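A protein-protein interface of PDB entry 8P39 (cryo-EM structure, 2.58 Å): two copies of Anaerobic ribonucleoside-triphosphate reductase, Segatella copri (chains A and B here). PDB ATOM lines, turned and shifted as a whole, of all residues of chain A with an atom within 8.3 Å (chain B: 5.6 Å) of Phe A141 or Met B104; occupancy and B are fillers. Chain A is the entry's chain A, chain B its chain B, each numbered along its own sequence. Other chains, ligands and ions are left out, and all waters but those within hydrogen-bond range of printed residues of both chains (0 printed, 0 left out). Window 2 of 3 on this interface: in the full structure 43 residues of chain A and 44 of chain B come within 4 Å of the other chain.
Among the printed residues, merely in contact across the chains: Thr A137 with Phe B103 (3.5 Å), Phe A141 with Met B104 (3.6 Å), Pro A169 with Val B107 (3.7 Å) and Phe A141 with Phe B103 (3.98 Å).
No position is printed for both chains.
Hydrophobic or aromatic side chains of chain B within 4 Å of the printed part of chain A: Phe B103, Met B104 and Val B107. Hydrophobic or aromatic side chains of chain A that line the printed part of chain B: Phe A141, Tyr A145 and Pro A169. Among the printed residues, no Asp or Glu carboxylate lies within 4 Å of a Lys or Arg side-chain nitrogen of the other chain.
The guanidinium group (NE) of Arg B100 lies within salt-bridge range of the side-chain carboxylate (OD1) of Asp B101, 2.8 Å away.
Of the printed residues of chain B, Phe A141 touches Phe B103 (3.98 Å) and Met B104 (3.6 Å). Of chain A, only Phe A141 comes within 4 Å of Met B104. No residue of chain A comes within 4 Å of Ser B105. Of the printed residues of chain A, Val B107 touches Pro A169 (3.7 Å). Of the printed residues of chain B, Pro A169 touches Val B107 (3.7 Å). Printed residues of chain A within 4 Å of Arg B100: Tyr A145 (2.8 Å). Of the printed residues of chain B, Thr A137 touches Phe B103. Printed residues of chain B within 4 Å of Tyr A145: Arg B100. The nearest printed residue of chain B that does not touch Phe A141 is Arg B100 (4.5 Å). The nearest residue of chain A that does not touch Met B104 is Leu A146 (5.2 Å). The nearest printed residue of chain A that does not touch Phe B103 is Thr A138 (6.0 Å).
The guanidinium group (NH1) of Arg B100 sits at hydrogen-bond distance from the side-chain hydroxyl (OH) of Tyr A145 (2.8 Å).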
ATOM      1  N   ALA A 134      -8.910  36.965   6.692  1.00  0.00           N
ATOM      2  CA  ALA A 134      -9.290  36.428   7.993  1.00  0.00           C
ATOM      3  C   ALA A 134     -10.532  35.552   7.889  1.00  0.00           C
ATOM      4  O   ALA A 134     -10.611  34.497   8.528  1.00  0.00           O
ATOM      5  CB  ALA A 134      -9.523  37.565   8.983  1.00  0.00           C
ATOM      6  N   SER A 135     -11.513  35.975   7.087  1.00  0.00           N
ATOM      7  CA  SER A 135     -12.757  35.220   6.971  1.00  0.00           C
ATOM      8  C   SER A 135     -12.524  33.849   6.349  1.00  0.00           C
ATOM      9  O   SER A 135     -13.019  32.839   6.861  1.00  0.00           O
ATOM     10  CB  SER A 135     -13.777  36.013   6.156  1.00  0.00           C
ATOM     11  OG  SER A 135     -14.079  37.250   6.780  1.00  0.00           O
ATOM     12  N   GLU A 136     -11.770  33.790   5.249  1.00  0.00           N
ATOM     13  CA  GLU A 136     -11.488  32.510   4.608  1.00  0.00           C
ATOM     14  C   GLU A 136     -10.566  31.636   5.445  1.00  0.00           C
ATOM     15  O   GLU A 136     -10.409  30.451   5.138  1.00  0.00           O
ATOM     16  CB  GLU A 136     -10.880  32.731   3.225  1.00  0.00           C
ATOM     17  CG  GLU A 136     -11.845  33.339   2.223  1.00  0.00           C
ATOM     18  CD  GLU A 136     -11.232  33.511   0.849  1.00  0.00           C
ATOM     19  OE1 GLU A 136     -10.049  33.149   0.673  1.00  0.00           O
ATOM     20  OE2 GLU A 136     -11.933  34.011  -0.056  1.00  0.00           O
ATOM     21  N   THR A 137      -9.949  32.197   6.485  1.00  0.00           N
ATOM     22  CA  THR A 137      -9.126  31.396   7.383  1.00  0.00           C
ATOM     23  C   THR A 137      -9.947  30.865   8.551  1.00  0.00           C
ATOM     24  O   THR A 137      -9.857  29.681   8.901  1.00  0.00           O
ATOM     25  CB  THR A 137      -7.945  32.226   7.889  1.00  0.00           C
ATOM     26  OG1 THR A 137      -7.018  32.442   6.820  1.00  0.00           O
ATOM     27  CG2 THR A 137      -7.245  31.519   9.032  1.00  0.00           C
ATOM     28  N   THR A 138     -10.764  31.722   9.159  1.00  0.00           N
ATOM     29  CA  THR A 138     -11.507  31.360  10.357  1.00  0.00           C
ATOM     30  C   THR A 138     -12.818  30.639  10.069  1.00  0.00           C
ATOM     31  O   THR A 138     -13.413  30.084  10.998  1.00  0.00           O
ATOM     32  CB  THR A 138     -11.796  32.612  11.195  1.00  0.00           C
ATOM     33  OG1 THR A 138     -12.276  32.223  12.486  1.00  0.00           O
ATOM     34  CG2 THR A 138     -12.847  33.475  10.516  1.00  0.00           C
ATOM     35  N   LYS A 139     -13.285  30.628   8.820  1.00  0.00           N
ATOM     36  CA  LYS A 139     -14.542  29.962   8.491  1.00  0.00           C
ATOM     37  C   LYS A 139     -14.366  28.446   8.386  1.00  0.00           C
ATOM     38  O   LYS A 139     -15.182  27.704   8.948  1.00  0.00           O
ATOM     39  CB  LYS A 139     -15.140  30.529   7.201  1.00  0.00           C
ATOM     40  CG  LYS A 139     -16.485  29.935   6.833  1.00  0.00           C
ATOM     41  CD  LYS A 139     -17.021  30.533   5.544  1.00  0.00           C
ATOM     42  CE  LYS A 139     -17.239  32.025   5.678  1.00  0.00           C
ATOM     43  NZ  LYS A 139     -17.786  32.614   4.426  1.00  0.00           N
ATOM     44  N   PRO A 140     -13.350  27.931   7.679  1.00  0.00           N
ATOM     45  CA  PRO A 140     -13.106  26.481   7.734  1.00  0.00           C
ATOM     46  C   PRO A 140     -12.591  26.009   9.080  1.00  0.00           C
ATOM     47  O   PRO A 140     -12.627  24.802   9.349  1.00  0.00           O
ATOM     48  CB  PRO A 140     -12.069  26.253   6.628  1.00  0.00           C
ATOM     49  CG  PRO A 140     -11.370  27.547   6.508  1.00  0.00           C
ATOM     50  CD  PRO A 140     -12.425  28.586   6.734  1.00  0.00           C
ATOM     51  N   PHE A 141     -12.113  26.916   9.932  1.00  0.00           N
ATOM     52  CA  PHE A 141     -11.616  26.518  11.244  1.00  0.00           C
ATOM     53  C   PHE A 141     -12.751  26.125  12.180  1.00  0.00           C
ATOM     54  O   PHE A 141     -12.663  25.108  12.878  1.00  0.00           O
ATOM     55  CB  PHE A 141     -10.792  27.653  11.850  1.00  0.00           C
ATOM     56  CG  PHE A 141     -10.380  27.415  13.271  1.00  0.00           C
ATOM     57  CD1 PHE A 141      -9.275  26.638  13.563  1.00  0.00           C
ATOM     58  CD2 PHE A 141     -11.085  27.988  14.315  1.00  0.00           C
ATOM     59  CE1 PHE A 141      -8.888  26.423  14.872  1.00  0.00           C
ATOM     60  CE2 PHE A 141     -10.702  27.778  15.625  1.00  0.00           C
ATOM     61  CZ  PHE A 141      -9.604  26.995  15.903  1.00  0.00           C
ATOM     62  N   VAL A 142     -13.823  26.921  12.215  1.00  0.00           N
ATOM     63  CA  VAL A 142     -14.897  26.692  13.176  1.00  0.00           C
ATOM     64  C   VAL A 142     -15.678  25.420  12.876  1.00  0.00           C
ATOM     65  O   VAL A 142     -16.322  24.870  13.777  1.00  0.00           O
ATOM     66  CB  VAL A 142     -15.846  27.905  13.223  1.00  0.00           C
ATOM     67  CG1 VAL A 142     -15.088  29.157  13.637  1.00  0.00           C
ATOM     68  CG2 VAL A 142     -16.519  28.105  11.877  1.00  0.00           C
ATOM     69  N   ASP A 143     -15.645  24.939  11.631  1.00  0.00           N
ATOM     70  CA  ASP A 143     -16.394  23.737  11.284  1.00  0.00           C
ATOM     71  C   ASP A 143     -15.913  22.522  12.065  1.00  0.00           C
ATOM     72  O   ASP A 143     -16.733  21.725  12.533  1.00  0.00           O
ATOM     73  CB  ASP A 143     -16.295  23.464   9.784  1.00  0.00           C
ATOM     74  CG  ASP A 143     -17.127  24.423   8.963  1.00  0.00           C
ATOM     75  OD1 ASP A 143     -17.811  25.281   9.560  1.00  0.00           O
ATOM     76  OD2 ASP A 143     -17.101  24.318   7.719  1.00  0.00           O
ATOM     77  N   ASP A 144     -14.602  22.363  12.221  1.00  0.00           N
ATOM     78  CA  ASP A 144     -14.020  21.183  12.854  1.00  0.00           C
ATOM     79  C   ASP A 144     -13.017  21.613  13.922  1.00  0.00           C
ATOM     80  O   ASP A 144     -11.815  21.652  13.653  1.00  0.00           O
ATOM     81  CB  ASP A 144     -13.368  20.293  11.806  1.00  0.00           C
ATOM     82  CG  ASP A 144     -12.625  21.088  10.756  1.00  0.00           C
ATOM     83  OD1 ASP A 144     -13.134  22.152  10.351  1.00  0.00           O
ATOM     84  OD2 ASP A 144     -11.531  20.655  10.338  1.00  0.00           O
ATOM     85  N   TYR A 145     -13.533  21.884  15.128  1.00  0.00           N
ATOM     86  CA  TYR A 145     -12.795  22.231  16.344  1.00  0.00           C
ATOM     87  C   TYR A 145     -13.712  22.957  17.319  1.00  0.00           C
ATOM     88  O   TYR A 145     -13.330  23.219  18.463  1.00  0.00           O
ATOM     89  CB  TYR A 145     -11.569  23.107  16.062  1.00  0.00           C
ATOM     90  CG  TYR A 145     -10.267  22.335  16.064  1.00  0.00           C
ATOM     91  CD1 TYR A 145     -10.019  21.363  17.024  1.00  0.00           C
ATOM     92  CD2 TYR A 145      -9.293  22.567  15.100  1.00  0.00           C
ATOM     93  CE1 TYR A 145      -8.837  20.652  17.030  1.00  0.00           C
ATOM     94  CE2 TYR A 145      -8.108  21.858  15.097  1.00  0.00           C
ATOM     95  CZ  TYR A 145      -7.885  20.903  16.065  1.00  0.00           C
ATOM     96  OH  TYR A 145      -6.706  20.194  16.070  1.00  0.00           O
ATOM     97  N   LEU A 146     -14.927  23.282  16.876  1.00  0.00           N
ATOM     98  CA  LEU A 146     -15.897  23.971  17.723  1.00  0.00           C
ATOM     99  C   LEU A 146     -17.295  23.369  17.692  1.00  0.00           C
ATOM    100  O   LEU A 146     -18.058  23.597  18.636  1.00  0.00           O
ATOM    101  CB  LEU A 146     -15.987  25.452  17.333  1.00  0.00           C
ATOM    102  CG  LEU A 146     -14.708  26.270  17.521  1.00  0.00           C
ATOM    103  CD1 LEU A 146     -14.881  27.679  16.985  1.00  0.00           C
ATOM    104  CD2 LEU A 146     -14.300  26.297  18.987  1.00  0.00           C
ATOM    105  N   LEU A 147     -17.664  22.615  16.662  1.00  0.00           N
ATOM    106  CA  LEU A 147     -18.994  22.039  16.560  1.00  0.00           C
ATOM    107  C   LEU A 147     -18.980  20.569  16.964  1.00  0.00           C
ATOM    108  O   LEU A 147     -17.990  19.858  16.771  1.00  0.00           O
ATOM    109  CB  LEU A 147     -19.532  22.177  15.135  1.00  0.00           C
ATOM    110  CG  LEU A 147     -19.538  23.567  14.497  1.00  0.00           C
ATOM    111  CD1 LEU A 147     -20.016  23.483  13.057  1.00  0.00           C
ATOM    112  CD2 LEU A 147     -20.405  24.524  15.295  1.00  0.00           C
ATOM    113  N   ARG A 152     -22.386  19.136  13.239  1.00  0.00           N
ATOM    114  CA  ARG A 152     -21.514  19.198  12.070  1.00  0.00           C
ATOM    115  C   ARG A 152     -22.169  18.542  10.863  1.00  0.00           C
ATOM    116  O   ARG A 152     -22.175  19.104   9.763  1.00  0.00           O
ATOM    117  CB  ARG A 152     -20.174  18.522  12.365  1.00  0.00           C
ATOM    118  CG  ARG A 152     -19.125  19.416  12.993  1.00  0.00           C
ATOM    119  CD  ARG A 152     -17.752  18.758  12.962  1.00  0.00           C
ATOM    120  NE  ARG A 152     -17.166  18.781  11.627  1.00  0.00           N
ATOM    121  CZ  ARG A 152     -17.226  17.779  10.761  1.00  0.00           C
ATOM    122  NH1 ARG A 152     -17.834  16.643  11.058  1.00  0.00           N
ATOM    123  NH2 ARG A 152     -16.657  17.920   9.567  1.00  0.00           N
ATOM    124  N   LYS A 165     -20.959  33.290  10.593  1.00  0.00           N
ATOM    125  CA  LYS A 165     -20.050  32.301  11.158  1.00  0.00           C
ATOM    126  C   LYS A 165     -18.599  32.765  11.153  1.00  0.00           C
ATOM    127  O   LYS A 165     -17.762  32.134  11.808  1.00  0.00           O
ATOM    128  CB  LYS A 165     -20.177  30.979  10.395  1.00  0.00           C
ATOM    129  CG  LYS A 165     -19.713  29.758  11.174  1.00  0.00           C
ATOM    130  CD  LYS A 165     -19.894  28.483  10.372  1.00  0.00           C
ATOM    131  CE  LYS A 165     -19.098  28.523   9.081  1.00  0.00           C
ATOM    132  NZ  LYS A 165     -19.279  27.281   8.284  1.00  0.00           N
ATOM    133  N   ASP A 166     -18.283  33.847  10.437  1.00  0.00           N
ATOM    134  CA  ASP A 166     -16.916  34.355  10.422  1.00  0.00           C
ATOM    135  C   ASP A 166     -16.492  34.840  11.802  1.00  0.00           C
ATOM    136  O   ASP A 166     -15.370  34.574  12.245  1.00  0.00           O
ATOM    137  CB  ASP A 166     -16.789  35.482   9.402  1.00  0.00           C
ATOM    138  CG  ASP A 166     -17.510  35.179   8.108  1.00  0.00           C
ATOM    139  OD1 ASP A 166     -18.132  34.101   8.016  1.00  0.00           O
ATOM    140  OD2 ASP A 166     -17.457  36.018   7.185  1.00  0.00           O
ATOM    141  N   TYR A 168     -17.420  33.812  14.610  1.00  0.00           N
ATOM    142  CA  TYR A 168     -17.650  32.797  15.636  1.00  0.00           C
ATOM    143  C   TYR A 168     -16.569  32.796  16.713  1.00  0.00           C
ATOM    144  O   TYR A 168     -16.923  32.813  17.904  1.00  0.00           O
ATOM    145  CB  TYR A 168     -17.785  31.425  14.960  1.00  0.00           C
ATOM    146  CG  TYR A 168     -18.550  30.367  15.735  1.00  0.00           C
ATOM    147  CD1 TYR A 168     -18.066  29.865  16.933  1.00  0.00           C
ATOM    148  CD2 TYR A 168     -19.738  29.844  15.239  1.00  0.00           C
ATOM    149  CE1 TYR A 168     -18.755  28.890  17.629  1.00  0.00           C
ATOM    150  CE2 TYR A 168     -20.431  28.869  15.928  1.00  0.00           C
ATOM    151  CZ  TYR A 168     -19.937  28.399  17.123  1.00  0.00           C
ATOM    152  OH  TYR A 168     -20.621  27.426  17.813  1.00  0.00           O
ATOM    153  N   PRO A 169     -15.267  32.774  16.394  1.00  0.00           N
ATOM    154  CA  PRO A 169     -14.263  32.827  17.472  1.00  0.00           C
ATOM    155  C   PRO A 169     -14.284  34.118  18.268  1.00  0.00           C
ATOM    156  O   PRO A 169     -13.940  34.108  19.456  1.00  0.00           O
ATOM    157  CB  PRO A 169     -12.936  32.652  16.722  1.00  0.00           C
ATOM    158  CG  PRO A 169     -13.308  32.005  15.440  1.00  0.00           C
ATOM    159  CD  PRO A 169     -14.622  32.600  15.081  1.00  0.00           C
ATOM    160  N   PHE A 488     -20.597  29.063  23.888  1.00  0.00           N
ATOM    161  CA  PHE A 488     -19.306  29.565  23.433  1.00  0.00           C
ATOM    162  C   PHE A 488     -19.173  31.063  23.688  1.00  0.00           C
ATOM    163  O   PHE A 488     -18.107  31.537  24.096  1.00  0.00           O
ATOM    164  CB  PHE A 488     -19.125  29.243  21.948  1.00  0.00           C
ATOM    165  CG  PHE A 488     -17.728  29.461  21.439  1.00  0.00           C
ATOM    166  CD1 PHE A 488     -16.666  28.736  21.953  1.00  0.00           C
ATOM    167  CD2 PHE A 488     -17.481  30.372  20.429  1.00  0.00           C
ATOM    168  CE1 PHE A 488     -15.382  28.932  21.481  1.00  0.00           C
ATOM    169  CE2 PHE A 488     -16.199  30.567  19.951  1.00  0.00           C
ATOM    170  CZ  PHE A 488     -15.150  29.846  20.478  1.00  0.00           C
ATOM    171  N   ARG B 100      -2.715  25.462  14.863  1.00  0.00           N
ATOM    172  CA  ARG B 100      -3.932  25.449  15.661  1.00  0.00           C
ATOM    173  C   ARG B 100      -3.755  26.135  17.005  1.00  0.00           C
ATOM    174  O   ARG B 100      -4.682  26.790  17.488  1.00  0.00           O
ATOM    175  CB  ARG B 100      -4.400  24.003  15.877  1.00  0.00           C
ATOM    176  CG  ARG B 100      -5.689  23.838  16.674  1.00  0.00           C
ATOM    177  CD  ARG B 100      -5.420  23.583  18.154  1.00  0.00           C
ATOM    178  NE  ARG B 100      -4.444  22.520  18.364  1.00  0.00           N
ATOM    179  CZ  ARG B 100      -4.754  21.250  18.594  1.00  0.00           C
ATOM    180  NH1 ARG B 100      -6.012  20.846  18.652  1.00  0.00           N
ATOM    181  NH2 ARG B 100      -3.776  20.367  18.773  1.00  0.00           N
ATOM    182  N   ASP B 101      -2.579  25.997  17.616  1.00  0.00           N
ATOM    183  CA  ASP B 101      -2.298  26.686  18.867  1.00  0.00           C
ATOM    184  C   ASP B 101      -2.063  28.176  18.663  1.00  0.00           C
ATOM    185  O   ASP B 101      -2.114  28.938  19.634  1.00  0.00           O
ATOM    186  CB  ASP B 101      -1.084  26.054  19.550  1.00  0.00           C
ATOM    187  CG  ASP B 101      -1.220  24.551  19.700  1.00  0.00           C
ATOM    188  OD1 ASP B 101      -2.247  23.999  19.255  1.00  0.00           O
ATOM    189  OD2 ASP B 101      -0.299  23.923  20.261  1.00  0.00           O
ATOM    190  N   VAL B 102      -1.801  28.606  17.428  1.00  0.00           N
ATOM    191  CA  VAL B 102      -1.633  30.022  17.119  1.00  0.00           C
ATOM    192  C   VAL B 102      -2.987  30.716  17.185  1.00  0.00           C
ATOM    193  O   VAL B 102      -3.129  31.765  17.823  1.00  0.00           O
ATOM    194  CB  VAL B 102      -0.976  30.222  15.740  1.00  0.00           C
ATOM    195  CG1 VAL B 102      -1.144  31.658  15.273  1.00  0.00           C
ATOM    196  CG2 VAL B 102       0.497  29.860  15.798  1.00  0.00           C
ATOM    197  N   PHE B 103      -3.993  30.129  16.531  1.00  0.00           N
ATOM    198  CA  PHE B 103      -5.324  30.725  16.510  1.00  0.00           C
ATOM    199  C   PHE B 103      -5.951  30.743  17.897  1.00  0.00           C
ATOM    200  O   PHE B 103      -6.594  31.721  18.290  1.00  0.00           O
ATOM    201  CB  PHE B 103      -6.220  29.972  15.524  1.00  0.00           C
ATOM    202  CG  PHE B 103      -5.786  30.096  14.093  1.00  0.00           C
ATOM    203  CD1 PHE B 103      -4.871  31.062  13.710  1.00  0.00           C
ATOM    204  CD2 PHE B 103      -6.296  29.247  13.127  1.00  0.00           C
ATOM    205  CE1 PHE B 103      -4.469  31.176  12.396  1.00  0.00           C
ATOM    206  CE2 PHE B 103      -5.899  29.356  11.809  1.00  0.00           C
ATOM    207  CZ  PHE B 103      -4.984  30.322  11.444  1.00  0.00           C
ATOM    208  N   MET B 104      -5.772  29.660  18.655  1.00  0.00           N
ATOM    209  CA  MET B 104      -6.284  29.579  20.017  1.00  0.00           C
ATOM    210  C   MET B 104      -5.669  30.664  20.890  1.00  0.00           C
ATOM    211  O   MET B 104      -6.350  31.244  21.741  1.00  0.00           O
ATOM    212  CB  MET B 104      -6.013  28.196  20.615  1.00  0.00           C
ATOM    213  CG  MET B 104      -6.897  27.080  20.067  1.00  0.00           C
ATOM    214  SD  MET B 104      -8.612  27.155  20.635  1.00  0.00           S
ATOM    215  CE  MET B 104      -9.401  28.048  19.294  1.00  0.00           C
ATOM    216  N   SER B 105      -4.380  30.940  20.686  1.00  0.00           N
ATOM    217  CA  SER B 105      -3.728  32.017  21.422  1.00  0.00           C
ATOM    218  C   SER B 105      -4.355  33.368  21.108  1.00  0.00           C
ATOM    219  O   SER B 105      -4.507  34.208  22.001  1.00  0.00           O
ATOM    220  CB  SER B 105      -2.232  32.038  21.108  1.00  0.00           C
ATOM    221  OG  SER B 105      -2.004  32.213  19.721  1.00  0.00           O
ATOM    222  N   ILE B 106      -4.714  33.598  19.843  1.00  0.00           N
ATOM    223  CA  ILE B 106      -5.390  34.837  19.470  1.00  0.00           C
ATOM    224  C   ILE B 106      -6.779  34.900  20.095  1.00  0.00           C
ATOM    225  O   ILE B 106      -7.188  35.938  20.631  1.00  0.00           O
ATOM    226  CB  ILE B 106      -5.452  34.964  17.936  1.00  0.00           C
ATOM    227  CG1 ILE B 106      -4.042  35.070  17.353  1.00  0.00           C
ATOM    228  CG2 ILE B 106      -6.299  36.158  17.529  1.00  0.00           C
ATOM    229  CD1 ILE B 106      -4.007  35.109  15.843  1.00  0.00           C
ATOM    230  N   VAL B 107      -7.523  33.793  20.042  1.00  0.00           N
ATOM    231  CA  VAL B 107      -8.897  33.783  20.536  1.00  0.00           C
ATOM    232  C   VAL B 107      -8.937  34.027  22.040  1.00  0.00           C
ATOM    233  O   VAL B 107      -9.768  34.798  22.534  1.00  0.00           O
ATOM    234  CB  VAL B 107      -9.585  32.459  20.157  1.00  0.00           C
ATOM    235  CG1 VAL B 107     -10.935  32.340  20.843  1.00  0.00           C
ATOM    236  CG2 VAL B 107      -9.741  32.359  18.648  1.00  0.00           C
ATOM    237  N   ASN B 108      -8.043  33.387  22.790  1.00  0.00           N
ATOM    238  CA  ASN B 108      -8.064  33.452  24.247  1.00  0.00           C
ATOM    239  C   ASN B 108      -7.513  34.762  24.801  1.00  0.00           C
ATOM    240  O   ASN B 108      -7.395  34.891  26.025  1.00  0.00           O
ATOM    241  CB  ASN B 108      -7.284  32.274  24.835  1.00  0.00           C
ATOM    242  CG  ASN B 108      -7.971  30.945  24.598  1.00  0.00           C
ATOM    243  OD1 ASN B 108      -8.723  30.463  25.443  1.00  0.00           O
ATOM    244  ND2 ASN B 108      -7.713  30.343  23.443  1.00  0.00           N
ATOM    245  N   ALA B 109      -7.179  35.722  23.937  1.00  0.00           N
ATOM    246  CA  ALA B 109      -6.658  37.028  24.345  1.00  0.00           C
ATOM    247  C   ALA B 109      -5.388  36.874  25.184  1.00  0.00           C
ATOM    248  O   ALA B 109      -5.321  37.272  26.349  1.00  0.00           O
ATOM    249  CB  ALA B 109      -7.725  37.837  25.091  1.00  0.00           C
ATOM    250  N   LYS B 110      -4.372  36.283  24.561  1.00  0.00           N
ATOM    251  CA  LYS B 110      -3.084  36.085  25.205  1.00  0.00           C
ATOM    252  C   LYS B 110      -2.291  37.391  25.209  1.00  0.00           C
ATOM    253  O   LYS B 110      -2.738  38.425  24.702  1.00  0.00           O
ATOM    254  CB  LYS B 110      -2.316  34.964  24.509  1.00  0.00           C
ATOM    255  CG  LYS B 110      -2.860  33.572  24.787  1.00  0.00           C
ATOM    256  CD  LYS B 110      -2.589  33.164  26.226  1.00  0.00           C
ATOM    257  CE  LYS B 110      -3.062  31.748  26.511  1.00  0.00           C
ATOM    258  NZ  LYS B 110      -4.543  31.636  26.479  1.00  0.00           N
